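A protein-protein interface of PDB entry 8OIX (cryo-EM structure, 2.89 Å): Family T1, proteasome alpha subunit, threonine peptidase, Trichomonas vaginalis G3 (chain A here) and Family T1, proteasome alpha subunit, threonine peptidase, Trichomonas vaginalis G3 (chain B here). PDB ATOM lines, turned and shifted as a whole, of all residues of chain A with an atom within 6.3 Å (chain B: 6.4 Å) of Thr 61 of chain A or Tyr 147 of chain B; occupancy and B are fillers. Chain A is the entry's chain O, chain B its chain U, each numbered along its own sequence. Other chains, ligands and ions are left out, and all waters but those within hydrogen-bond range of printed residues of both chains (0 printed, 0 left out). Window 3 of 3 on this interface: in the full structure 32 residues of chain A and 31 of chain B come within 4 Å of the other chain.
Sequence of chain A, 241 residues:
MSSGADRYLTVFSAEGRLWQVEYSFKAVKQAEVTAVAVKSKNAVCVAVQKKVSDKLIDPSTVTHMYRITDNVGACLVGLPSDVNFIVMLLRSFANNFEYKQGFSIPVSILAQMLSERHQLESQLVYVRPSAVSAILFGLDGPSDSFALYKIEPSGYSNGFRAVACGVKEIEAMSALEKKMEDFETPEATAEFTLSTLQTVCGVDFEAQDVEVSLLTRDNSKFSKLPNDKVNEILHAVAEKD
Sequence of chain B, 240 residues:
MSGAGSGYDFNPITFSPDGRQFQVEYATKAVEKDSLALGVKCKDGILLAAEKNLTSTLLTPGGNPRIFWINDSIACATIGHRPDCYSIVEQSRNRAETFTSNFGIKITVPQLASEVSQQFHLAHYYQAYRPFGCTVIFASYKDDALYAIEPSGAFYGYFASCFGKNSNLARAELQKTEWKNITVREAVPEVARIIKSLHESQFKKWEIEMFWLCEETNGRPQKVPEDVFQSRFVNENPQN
CB of Tyr 156 of chain B touches CG2 of Ile 57 of chain A (3.6 Å).
Ile 57 of chain A touches Gly 157 of chain B (CG2 to O, 3.2 Å).
Ile 57 of chain A touches Tyr 158 of chain B.
Asp 58 of chain A touches Tyr 158 of chain B.
Thr 61 of chain A touches Tyr 147 of chain B (CG2 to OH, 3.2 Å).
OG1 of Thr 61 of chain A touches C of Tyr 156 of chain B, 3.9 Å away.
Val 62 of chain A touches Tyr 156 of chain B.
Printed residues of chain B within 4 Å of Ile 57 of chain A: Tyr 156 (3.6 Å), Gly 157 (3.2 Å) and Tyr 158 (3.4 Å).
Thr 61 of chain A touches just these residues of chain B: Tyr 147 (3.2 Å), Tyr 156 (3.9 Å) and Gly 157 (2.9 Å).
Tyr 147 of chain B touches one residue of chain A.
Of the printed residues of chain A, Tyr 156 of chain B touches Ile 57 (3.6 Å), Thr 61 (3.9 Å) and Val 62 (3.7 Å).
Printed residues of chain A within 4 Å of Gly 157 of chain B: Ile 57, Asp 58 and Thr 61.
The nearest residue of chain A that does not touch Tyr 147 of chain B is Asp 58 of chain A (5.2 Å).
The nearest printed residue of chain B that does not touch Ile 57 of chain A is Ser 161 of chain B (6.9 Å).
The backbone carbonyl oxygen of Leu 146 of chain B sits at hydrogen-bond distance from the backbone NH of Tyr 158 of chain B, 2.6 Å away.
The side-chain carboxylate (OD2) of Asp 58 of chain A is in hydrogen-bond range of the side-chain hydroxyl (OG) of Ser 60 of chain A (2.8 Å).
The side-chain amino group (NZ) of Lys 50 of chain A sits at hydrogen-bond distance from the backbone carbonyl oxygen (O) of Val 62 of chain A (2.7 Å).
The backbone NH of Phe 138 of chain B lies within hydrogen-bond range of the backbone carbonyl oxygen of Tyr 147 of chain B (2.8 Å).
The backbone carbonyl oxygen of Asp 58 of chain A lies within hydrogen-bond range of the side-chain hydroxyl of Thr 61 of chain A (2.6 Å).
N of Ala 148 of chain B lies within hydrogen-bond range of O of Tyr 156 of chain B.
Hydrophobic or aromatic side chains of chain B within 4 Å of the printed part of chain A: Tyr 147, Tyr 156 and Tyr 158.
Along chain B the printed residues that touch a printed residue of chain A span positions 147 to 158.
Printed residues of chain A that touch a printed residue of chain B: Ile 57, Asp 58, Thr 61 and Val 62.
Hydrophobic or aromatic side chains of chain A that line the printed part of chain B: Ile 57 and Val 62.
O of Gly 157 of chain B is in hydrogen-bond range of N of Asp 58 of chain A (2.7 Å).
The side-chain hydroxyl (OG1) of Thr 61 of chain A sits at hydrogen-bond distance from the backbone NH (N) of Gly 157 of chain B (2.9 Å).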
ATOM      1  N   LYS A  50      24.121 -36.972 -40.020  1.00  0.00           N
ATOM      2  CA  LYS A  50      24.229 -36.090 -38.862  1.00  0.00           C
ATOM      3  C   LYS A  50      24.503 -34.675 -39.365  1.00  0.00           C
ATOM      4  O   LYS A  50      25.643 -34.220 -39.451  1.00  0.00           O
ATOM      5  CB  LYS A  50      25.322 -36.589 -37.924  1.00  0.00           C
ATOM      6  CG  LYS A  50      25.469 -35.803 -36.640  1.00  0.00           C
ATOM      7  CD  LYS A  50      26.893 -35.906 -36.132  1.00  0.00           C
ATOM      8  CE  LYS A  50      26.963 -35.681 -34.641  1.00  0.00           C
ATOM      9  NZ  LYS A  50      26.293 -36.771 -33.883  1.00  0.00           N
ATOM     10  N   ILE A  57      27.114 -25.625 -32.191  1.00  0.00           N
ATOM     11  CA  ILE A  57      26.489 -26.696 -31.429  1.00  0.00           C
ATOM     12  C   ILE A  57      27.498 -27.813 -31.206  1.00  0.00           C
ATOM     13  O   ILE A  57      28.247 -28.190 -32.117  1.00  0.00           O
ATOM     14  CB  ILE A  57      25.245 -27.218 -32.167  1.00  0.00           C
ATOM     15  CG1 ILE A  57      24.344 -26.059 -32.587  1.00  0.00           C
ATOM     16  CG2 ILE A  57      24.467 -28.160 -31.281  1.00  0.00           C
ATOM     17  CD1 ILE A  57      23.187 -26.477 -33.464  1.00  0.00           C
ATOM     18  N   ASP A  58      27.528 -28.344 -29.994  1.00  0.00           N
ATOM     19  CA  ASP A  58      28.355 -29.506 -29.691  1.00  0.00           C
ATOM     20  C   ASP A  58      27.816 -30.708 -30.454  1.00  0.00           C
ATOM     21  O   ASP A  58      26.714 -31.178 -30.140  1.00  0.00           O
ATOM     22  CB  ASP A  58      28.360 -29.777 -28.187  1.00  0.00           C
ATOM     23  CG  ASP A  58      29.234 -30.958 -27.805  1.00  0.00           C
ATOM     24  OD1 ASP A  58      30.049 -31.402 -28.642  1.00  0.00           O
ATOM     25  OD2 ASP A  58      29.105 -31.446 -26.663  1.00  0.00           O
ATOM     26  N   PRO A  59      28.532 -31.226 -31.457  1.00  0.00           N
ATOM     27  CA  PRO A  59      27.949 -32.281 -32.303  1.00  0.00           C
ATOM     28  C   PRO A  59      27.562 -33.533 -31.540  1.00  0.00           C
ATOM     29  O   PRO A  59      26.635 -34.236 -31.957  1.00  0.00           O
ATOM     30  CB  PRO A  59      29.062 -32.567 -33.321  1.00  0.00           C
ATOM     31  CG  PRO A  59      29.932 -31.353 -33.297  1.00  0.00           C
ATOM     32  CD  PRO A  59      29.891 -30.863 -31.886  1.00  0.00           C
ATOM     33  N   SER A  60      28.229 -33.826 -30.421  1.00  0.00           N
ATOM     34  CA  SER A  60      27.907 -35.026 -29.659  1.00  0.00           C
ATOM     35  C   SER A  60      26.475 -35.015 -29.146  1.00  0.00           C
ATOM     36  O   SER A  60      25.938 -36.075 -28.810  1.00  0.00           O
ATOM     37  CB  SER A  60      28.878 -35.182 -28.490  1.00  0.00           C
ATOM     38  OG  SER A  60      28.740 -34.114 -27.570  1.00  0.00           O
ATOM     39  N   THR A  61      25.846 -33.842 -29.080  1.00  0.00           N
ATOM     40  CA  THR A  61      24.456 -33.735 -28.664  1.00  0.00           C
ATOM     41  C   THR A  61      23.481 -33.753 -29.832  1.00  0.00           C
ATOM     42  O   THR A  61      22.283 -33.964 -29.616  1.00  0.00           O
ATOM     43  CB  THR A  61      24.253 -32.453 -27.856  1.00  0.00           C
ATOM     44  OG1 THR A  61      24.583 -31.321 -28.670  1.00  0.00           O
ATOM     45  CG2 THR A  61      25.156 -32.462 -26.644  1.00  0.00           C
ATOM     46  N   VAL A  62      23.960 -33.538 -31.056  1.00  0.00           N
ATOM     47  CA  VAL A  62      23.109 -33.598 -32.245  1.00  0.00           C
ATOM     48  C   VAL A  62      23.122 -35.056 -32.688  1.00  0.00           C
ATOM     49  O   VAL A  62      23.909 -35.472 -33.537  1.00  0.00           O
ATOM     50  CB  VAL A  62      23.584 -32.650 -33.342  1.00  0.00           C
ATOM     51  CG1 VAL A  62      22.699 -32.776 -34.575  1.00  0.00           C
ATOM     52  CG2 VAL A  62      23.590 -31.223 -32.837  1.00  0.00           C
ATOM     53  N   THR A  63      22.238 -35.846 -32.090  1.00  0.00           N
ATOM     54  CA  THR A  63      22.206 -37.279 -32.315  1.00  0.00           C
ATOM     55  C   THR A  63      20.793 -37.716 -32.657  1.00  0.00           C
ATOM     56  O   THR A  63      19.823 -37.254 -32.051  1.00  0.00           O
ATOM     57  CB  THR A  63      22.711 -38.051 -31.087  1.00  0.00           C
ATOM     58  OG1 THR A  63      22.481 -39.453 -31.269  1.00  0.00           O
ATOM     59  CG2 THR A  63      22.011 -37.578 -29.820  1.00  0.00           C
ATOM     60  N   TYR A  66      20.067 -43.440 -30.423  1.00  0.00           N
ATOM     61  CA  TYR A  66      19.954 -43.428 -28.977  1.00  0.00           C
ATOM     62  C   TYR A  66      19.985 -44.846 -28.428  1.00  0.00           C
ATOM     63  O   TYR A  66      19.534 -45.796 -29.075  1.00  0.00           O
ATOM     64  CB  TYR A  66      18.669 -42.730 -28.544  1.00  0.00           C
ATOM     65  CG  TYR A  66      18.603 -41.286 -28.971  1.00  0.00           C
ATOM     66  CD1 TYR A  66      18.090 -40.932 -30.212  1.00  0.00           C
ATOM     67  CD2 TYR A  66      19.038 -40.274 -28.130  1.00  0.00           C
ATOM     68  CE1 TYR A  66      18.020 -39.614 -30.602  1.00  0.00           C
ATOM     69  CE2 TYR A  66      18.970 -38.953 -28.512  1.00  0.00           C
ATOM     70  CZ  TYR A  66      18.461 -38.629 -29.749  1.00  0.00           C
ATOM     71  OH  TYR A  66      18.393 -37.311 -30.136  1.00  0.00           O
ATOM     72  N   VAL B 109      23.727 -31.219 -16.368  1.00  0.00           N
ATOM     73  CA  VAL B 109      23.051 -30.372 -17.355  1.00  0.00           C
ATOM     74  C   VAL B 109      22.529 -31.158 -18.549  1.00  0.00           C
ATOM     75  O   VAL B 109      21.445 -30.830 -19.042  1.00  0.00           O
ATOM     76  CB  VAL B 109      23.956 -29.198 -17.753  1.00  0.00           C
ATOM     77  CG1 VAL B 109      23.512 -28.594 -19.071  1.00  0.00           C
ATOM     78  CG2 VAL B 109      23.903 -28.142 -16.686  1.00  0.00           C
ATOM     79  N   PRO B 110      23.227 -32.166 -19.087  1.00  0.00           N
ATOM     80  CA  PRO B 110      22.607 -32.946 -20.175  1.00  0.00           C
ATOM     81  C   PRO B 110      21.276 -33.572 -19.785  1.00  0.00           C
ATOM     82  O   PRO B 110      20.261 -33.360 -20.464  1.00  0.00           O
ATOM     83  CB  PRO B 110      23.670 -34.004 -20.491  1.00  0.00           C
ATOM     84  CG  PRO B 110      24.945 -33.382 -20.090  1.00  0.00           C
ATOM     85  CD  PRO B 110      24.644 -32.531 -18.899  1.00  0.00           C
ATOM     86  N   GLN B 111      21.243 -34.326 -18.688  1.00  0.00           N
ATOM     87  CA  GLN B 111      19.998 -34.977 -18.309  1.00  0.00           C
ATOM     88  C   GLN B 111      19.017 -34.018 -17.647  1.00  0.00           C
ATOM     89  O   GLN B 111      17.805 -34.232 -17.737  1.00  0.00           O
ATOM     90  CB  GLN B 111      20.285 -36.179 -17.411  1.00  0.00           C
ATOM     91  CG  GLN B 111      20.733 -35.862 -16.014  1.00  0.00           C
ATOM     92  CD  GLN B 111      20.971 -37.120 -15.213  1.00  0.00           C
ATOM     93  OE1 GLN B 111      20.175 -38.057 -15.263  1.00  0.00           O
ATOM     94  NE2 GLN B 111      22.075 -37.156 -14.476  1.00  0.00           N
ATOM     95  N   ALA B 113      18.640 -31.015 -18.858  1.00  0.00           N
ATOM     96  CA  ALA B 113      18.056 -30.476 -20.076  1.00  0.00           C
ATOM     97  C   ALA B 113      17.065 -31.454 -20.683  1.00  0.00           C
ATOM     98  O   ALA B 113      16.017 -31.047 -21.185  1.00  0.00           O
ATOM     99  CB  ALA B 113      19.154 -30.130 -21.078  1.00  0.00           C
ATOM    100  N   SER B 114      17.380 -32.749 -20.653  1.00  0.00           N
ATOM    101  CA  SER B 114      16.424 -33.740 -21.139  1.00  0.00           C
ATOM    102  C   SER B 114      15.137 -33.712 -20.316  1.00  0.00           C
ATOM    103  O   SER B 114      14.028 -33.695 -20.868  1.00  0.00           O
ATOM    104  CB  SER B 114      17.056 -35.130 -21.114  1.00  0.00           C
ATOM    105  OG  SER B 114      16.256 -36.067 -21.812  1.00  0.00           O
ATOM    106  N   VAL B 136      16.030 -21.849 -22.601  1.00  0.00           N
ATOM    107  CA  VAL B 136      16.807 -21.893 -21.365  1.00  0.00           C
ATOM    108  C   VAL B 136      18.160 -22.537 -21.636  1.00  0.00           C
ATOM    109  O   VAL B 136      18.231 -23.684 -22.090  1.00  0.00           O
ATOM    110  CB  VAL B 136      16.051 -22.622 -20.244  1.00  0.00           C
ATOM    111  CG1 VAL B 136      14.958 -21.721 -19.706  1.00  0.00           C
ATOM    112  CG2 VAL B 136      15.442 -23.908 -20.766  1.00  0.00           C
ATOM    113  N   ILE B 137      19.225 -21.796 -21.358  1.00  0.00           N
ATOM    114  CA  ILE B 137      20.596 -22.257 -21.530  1.00  0.00           C
ATOM    115  C   ILE B 137      21.107 -22.675 -20.155  1.00  0.00           C
ATOM    116  O   ILE B 137      21.439 -21.831 -19.322  1.00  0.00           O
ATOM    117  CB  ILE B 137      21.477 -21.172 -22.153  1.00  0.00           C
ATOM    118  CG1 ILE B 137      20.836 -20.633 -23.431  1.00  0.00           C
ATOM    119  CG2 ILE B 137      22.852 -21.719 -22.451  1.00  0.00           C
ATOM    120  CD1 ILE B 137      21.681 -19.610 -24.153  1.00  0.00           C
ATOM    121  N   PHE B 138      21.157 -23.980 -19.909  1.00  0.00           N
ATOM    122  CA  PHE B 138      21.723 -24.528 -18.685  1.00  0.00           C
ATOM    123  C   PHE B 138      23.227 -24.691 -18.858  1.00  0.00           C
ATOM    124  O   PHE B 138      23.684 -25.367 -19.787  1.00  0.00           O
ATOM    125  CB  PHE B 138      21.079 -25.869 -18.344  1.00  0.00           C
ATOM    126  CG  PHE B 138      19.621 -25.771 -18.051  1.00  0.00           C
ATOM    127  CD1 PHE B 138      19.179 -25.330 -16.819  1.00  0.00           C
ATOM    128  CD2 PHE B 138      18.690 -26.112 -19.010  1.00  0.00           C
ATOM    129  CE1 PHE B 138      17.833 -25.234 -16.552  1.00  0.00           C
ATOM    130  CE2 PHE B 138      17.346 -26.019 -18.745  1.00  0.00           C
ATOM    131  CZ  PHE B 138      16.918 -25.579 -17.519  1.00  0.00           C
ATOM    132  N   ALA B 139      23.991 -24.070 -17.966  1.00  0.00           N
ATOM    133  CA  ALA B 139      25.441 -24.144 -17.974  1.00  0.00           C
ATOM    134  C   ALA B 139      25.936 -24.765 -16.677  1.00  0.00           C
ATOM    135  O   ALA B 139      25.410 -24.476 -15.595  1.00  0.00           O
ATOM    136  CB  ALA B 139      26.060 -22.759 -18.158  1.00  0.00           C
ATOM    137  N   ASP B 143      29.927 -30.098 -15.027  1.00  0.00           N
ATOM    138  CA  ASP B 143      29.510 -31.031 -16.061  1.00  0.00           C
ATOM    139  C   ASP B 143      30.045 -30.652 -17.431  1.00  0.00           C
ATOM    140  O   ASP B 143      29.751 -31.351 -18.408  1.00  0.00           O
ATOM    141  CB  ASP B 143      27.981 -31.119 -16.109  1.00  0.00           C
ATOM    142  CG  ASP B 143      27.376 -31.456 -14.764  1.00  0.00           C
ATOM    143  OD1 ASP B 143      27.951 -32.303 -14.049  1.00  0.00           O
ATOM    144  OD2 ASP B 143      26.329 -30.872 -14.417  1.00  0.00           O
ATOM    145  N   ASP B 144      30.846 -29.586 -17.520  1.00  0.00           N
ATOM    146  CA  ASP B 144      31.366 -29.051 -18.775  1.00  0.00           C
ATOM    147  C   ASP B 144      30.276 -29.045 -19.840  1.00  0.00           C
ATOM    148  O   ASP B 144      30.507 -29.447 -20.985  1.00  0.00           O
ATOM    149  CB  ASP B 144      32.582 -29.858 -19.240  1.00  0.00           C
ATOM    150  CG  ASP B 144      33.315 -29.199 -20.393  1.00  0.00           C
ATOM    151  OD1 ASP B 144      33.847 -28.085 -20.201  1.00  0.00           O
ATOM    152  OD2 ASP B 144      33.360 -29.793 -21.490  1.00  0.00           O
ATOM    153  N   ALA B 145      29.077 -28.612 -19.465  1.00  0.00           N
ATOM    154  CA  ALA B 145      27.912 -28.720 -20.327  1.00  0.00           C
ATOM    155  C   ALA B 145      27.256 -27.361 -20.496  1.00  0.00           C
ATOM    156  O   ALA B 145      27.108 -26.604 -19.531  1.00  0.00           O
ATOM    157  CB  ALA B 145      26.905 -29.724 -19.765  1.00  0.00           C
ATOM    158  N   LEU B 146      26.857 -27.063 -21.731  1.00  0.00           N
ATOM    159  CA  LEU B 146      26.104 -25.859 -22.072  1.00  0.00           C
ATOM    160  C   LEU B 146      24.965 -26.308 -22.983  1.00  0.00           C
ATOM    161  O   LEU B 146      25.101 -26.300 -24.208  1.00  0.00           O
ATOM    162  CB  LEU B 146      27.003 -24.832 -22.746  1.00  0.00           C
ATOM    163  CG  LEU B 146      26.409 -23.474 -23.105  1.00  0.00           C
ATOM    164  CD1 LEU B 146      26.198 -22.650 -21.853  1.00  0.00           C
ATOM    165  CD2 LEU B 146      27.312 -22.755 -24.082  1.00  0.00           C
ATOM    166  N   TYR B 147      23.844 -26.693 -22.382  1.00  0.00           N
ATOM    167  CA  TYR B 147      22.703 -27.231 -23.115  1.00  0.00           C
ATOM    168  C   TYR B 147      21.596 -26.190 -23.156  1.00  0.00           C
ATOM    169  O   TYR B 147      21.117 -25.751 -22.109  1.00  0.00           O
ATOM    170  CB  TYR B 147      22.194 -28.519 -22.471  1.00  0.00           C
ATOM    171  CG  TYR B 147      23.038 -29.738 -22.754  1.00  0.00           C
ATOM    172  CD1 TYR B 147      24.342 -29.827 -22.291  1.00  0.00           C
ATOM    173  CD2 TYR B 147      22.521 -30.811 -23.466  1.00  0.00           C
ATOM    174  CE1 TYR B 147      25.113 -30.941 -22.542  1.00  0.00           C
ATOM    175  CE2 TYR B 147      23.284 -31.930 -23.720  1.00  0.00           C
ATOM    176  CZ  TYR B 147      24.579 -31.991 -23.254  1.00  0.00           C
ATOM    177  OH  TYR B 147      25.346 -33.105 -23.504  1.00  0.00           O
ATOM    178  N   ALA B 148      21.167 -25.829 -24.355  1.00  0.00           N
ATOM    179  CA  ALA B 148      20.078 -24.885 -24.544  1.00  0.00           C
ATOM    180  C   ALA B 148      18.841 -25.639 -25.010  1.00  0.00           C
ATOM    181  O   ALA B 148      18.898 -26.389 -25.993  1.00  0.00           O
ATOM    182  CB  ALA B 148      20.462 -23.800 -25.549  1.00  0.00           C
ATOM    183  N   ILE B 149      17.752 -25.480 -24.261  1.00  0.00           N
ATOM    184  CA  ILE B 149      16.445 -26.020 -24.611  1.00  0.00           C
ATOM    185  C   ILE B 149      15.642 -24.922 -25.286  1.00  0.00           C
ATOM    186  O   ILE B 149      15.534 -23.808 -24.757  1.00  0.00           O
ATOM    187  CB  ILE B 149      15.705 -26.535 -23.366  1.00  0.00           C
ATOM    188  CG1 ILE B 149      16.627 -27.365 -22.483  1.00  0.00           C
ATOM    189  CG2 ILE B 149      14.488 -27.348 -23.775  1.00  0.00           C
ATOM    190  CD1 ILE B 149      15.936 -27.876 -21.254  1.00  0.00           C
ATOM    191  N   PHE B 155      16.658 -29.633 -27.292  1.00  0.00           N
ATOM    192  CA  PHE B 155      17.776 -29.200 -26.468  1.00  0.00           C
ATOM    193  C   PHE B 155      19.067 -29.722 -27.076  1.00  0.00           C
ATOM    194  O   PHE B 155      19.155 -30.895 -27.450  1.00  0.00           O
ATOM    195  CB  PHE B 155      17.622 -29.671 -25.014  1.00  0.00           C
ATOM    196  CG  PHE B 155      17.895 -31.133 -24.804  1.00  0.00           C
ATOM    197  CD1 PHE B 155      16.886 -32.065 -24.944  1.00  0.00           C
ATOM    198  CD2 PHE B 155      19.155 -31.570 -24.431  1.00  0.00           C
ATOM    199  CE1 PHE B 155      17.133 -33.406 -24.740  1.00  0.00           C
ATOM    200  CE2 PHE B 155      19.407 -32.910 -24.229  1.00  0.00           C
ATOM    201  CZ  PHE B 155      18.395 -33.828 -24.382  1.00  0.00           C
ATOM    202  N   TYR B 156      20.050 -28.840 -27.197  1.00  0.00           N
ATOM    203  CA  TYR B 156      21.355 -29.210 -27.727  1.00  0.00           C
ATOM    204  C   TYR B 156      22.454 -28.671 -26.832  1.00  0.00           C
ATOM    205  O   TYR B 156      22.336 -27.575 -26.287  1.00  0.00           O
ATOM    206  CB  TYR B 156      21.563 -28.678 -29.147  1.00  0.00           C
ATOM    207  CG  TYR B 156      20.571 -29.188 -30.158  1.00  0.00           C
ATOM    208  CD1 TYR B 156      20.685 -30.467 -30.678  1.00  0.00           C
ATOM    209  CD2 TYR B 156      19.528 -28.389 -30.602  1.00  0.00           C
ATOM    210  CE1 TYR B 156      19.787 -30.939 -31.606  1.00  0.00           C
ATOM    211  CE2 TYR B 156      18.623 -28.855 -31.530  1.00  0.00           C
ATOM    212  CZ  TYR B 156      18.759 -30.131 -32.028  1.00  0.00           C
ATOM    213  OH  TYR B 156      17.866 -30.606 -32.956  1.00  0.00           O
ATOM    214  N   GLY B 157      23.517 -29.453 -26.673  1.00  0.00           N
ATOM    215  CA  GLY B 157      24.730 -28.917 -26.092  1.00  0.00           C
ATOM    216  C   GLY B 157      25.437 -28.013 -27.086  1.00  0.00           C
ATOM    217  O   GLY B 157      25.504 -28.300 -28.282  1.00  0.00           O
ATOM    218  N   TYR B 158      25.963 -26.901 -26.586  1.00  0.00           N
ATOM    219  CA  TYR B 158      26.648 -25.928 -27.419  1.00  0.00           C
ATOM    220  C   TYR B 158      28.050 -25.672 -26.892  1.00  0.00           C
ATOM    221  O   TYR B 158      28.301 -25.746 -25.686  1.00  0.00           O
ATOM    222  CB  TYR B 158      25.898 -24.589 -27.475  1.00  0.00           C
ATOM    223  CG  TYR B 158      24.569 -24.608 -28.190  1.00  0.00           C
ATOM    224  CD1 TYR B 158      23.447 -25.165 -27.599  1.00  0.00           C
ATOM    225  CD2 TYR B 158      24.427 -24.032 -29.444  1.00  0.00           C
ATOM    226  CE1 TYR B 158      22.228 -25.173 -28.246  1.00  0.00           C
ATOM    227  CE2 TYR B 158      23.210 -24.031 -30.096  1.00  0.00           C
ATOM    228  CZ  TYR B 158      22.115 -24.605 -29.493  1.00  0.00           C
ATOM    229  OH  TYR B 158      20.901 -24.608 -30.139  1.00  0.00           O
ATOM    230  N   SER B 161      26.327 -20.942 -27.173  1.00  0.00           N
ATOM    231  CA  SER B 161      24.910 -20.820 -27.476  1.00  0.00           C
ATOM    232  C   SER B 161      24.482 -19.365 -27.364  1.00  0.00           C
ATOM    233  O   SER B 161      25.094 -18.581 -26.638  1.00  0.00           O
ATOM    234  CB  SER B 161      24.072 -21.676 -26.526  1.00  0.00           C
ATOM    235  OG  SER B 161      22.695 -21.589 -26.839  1.00  0.00           O
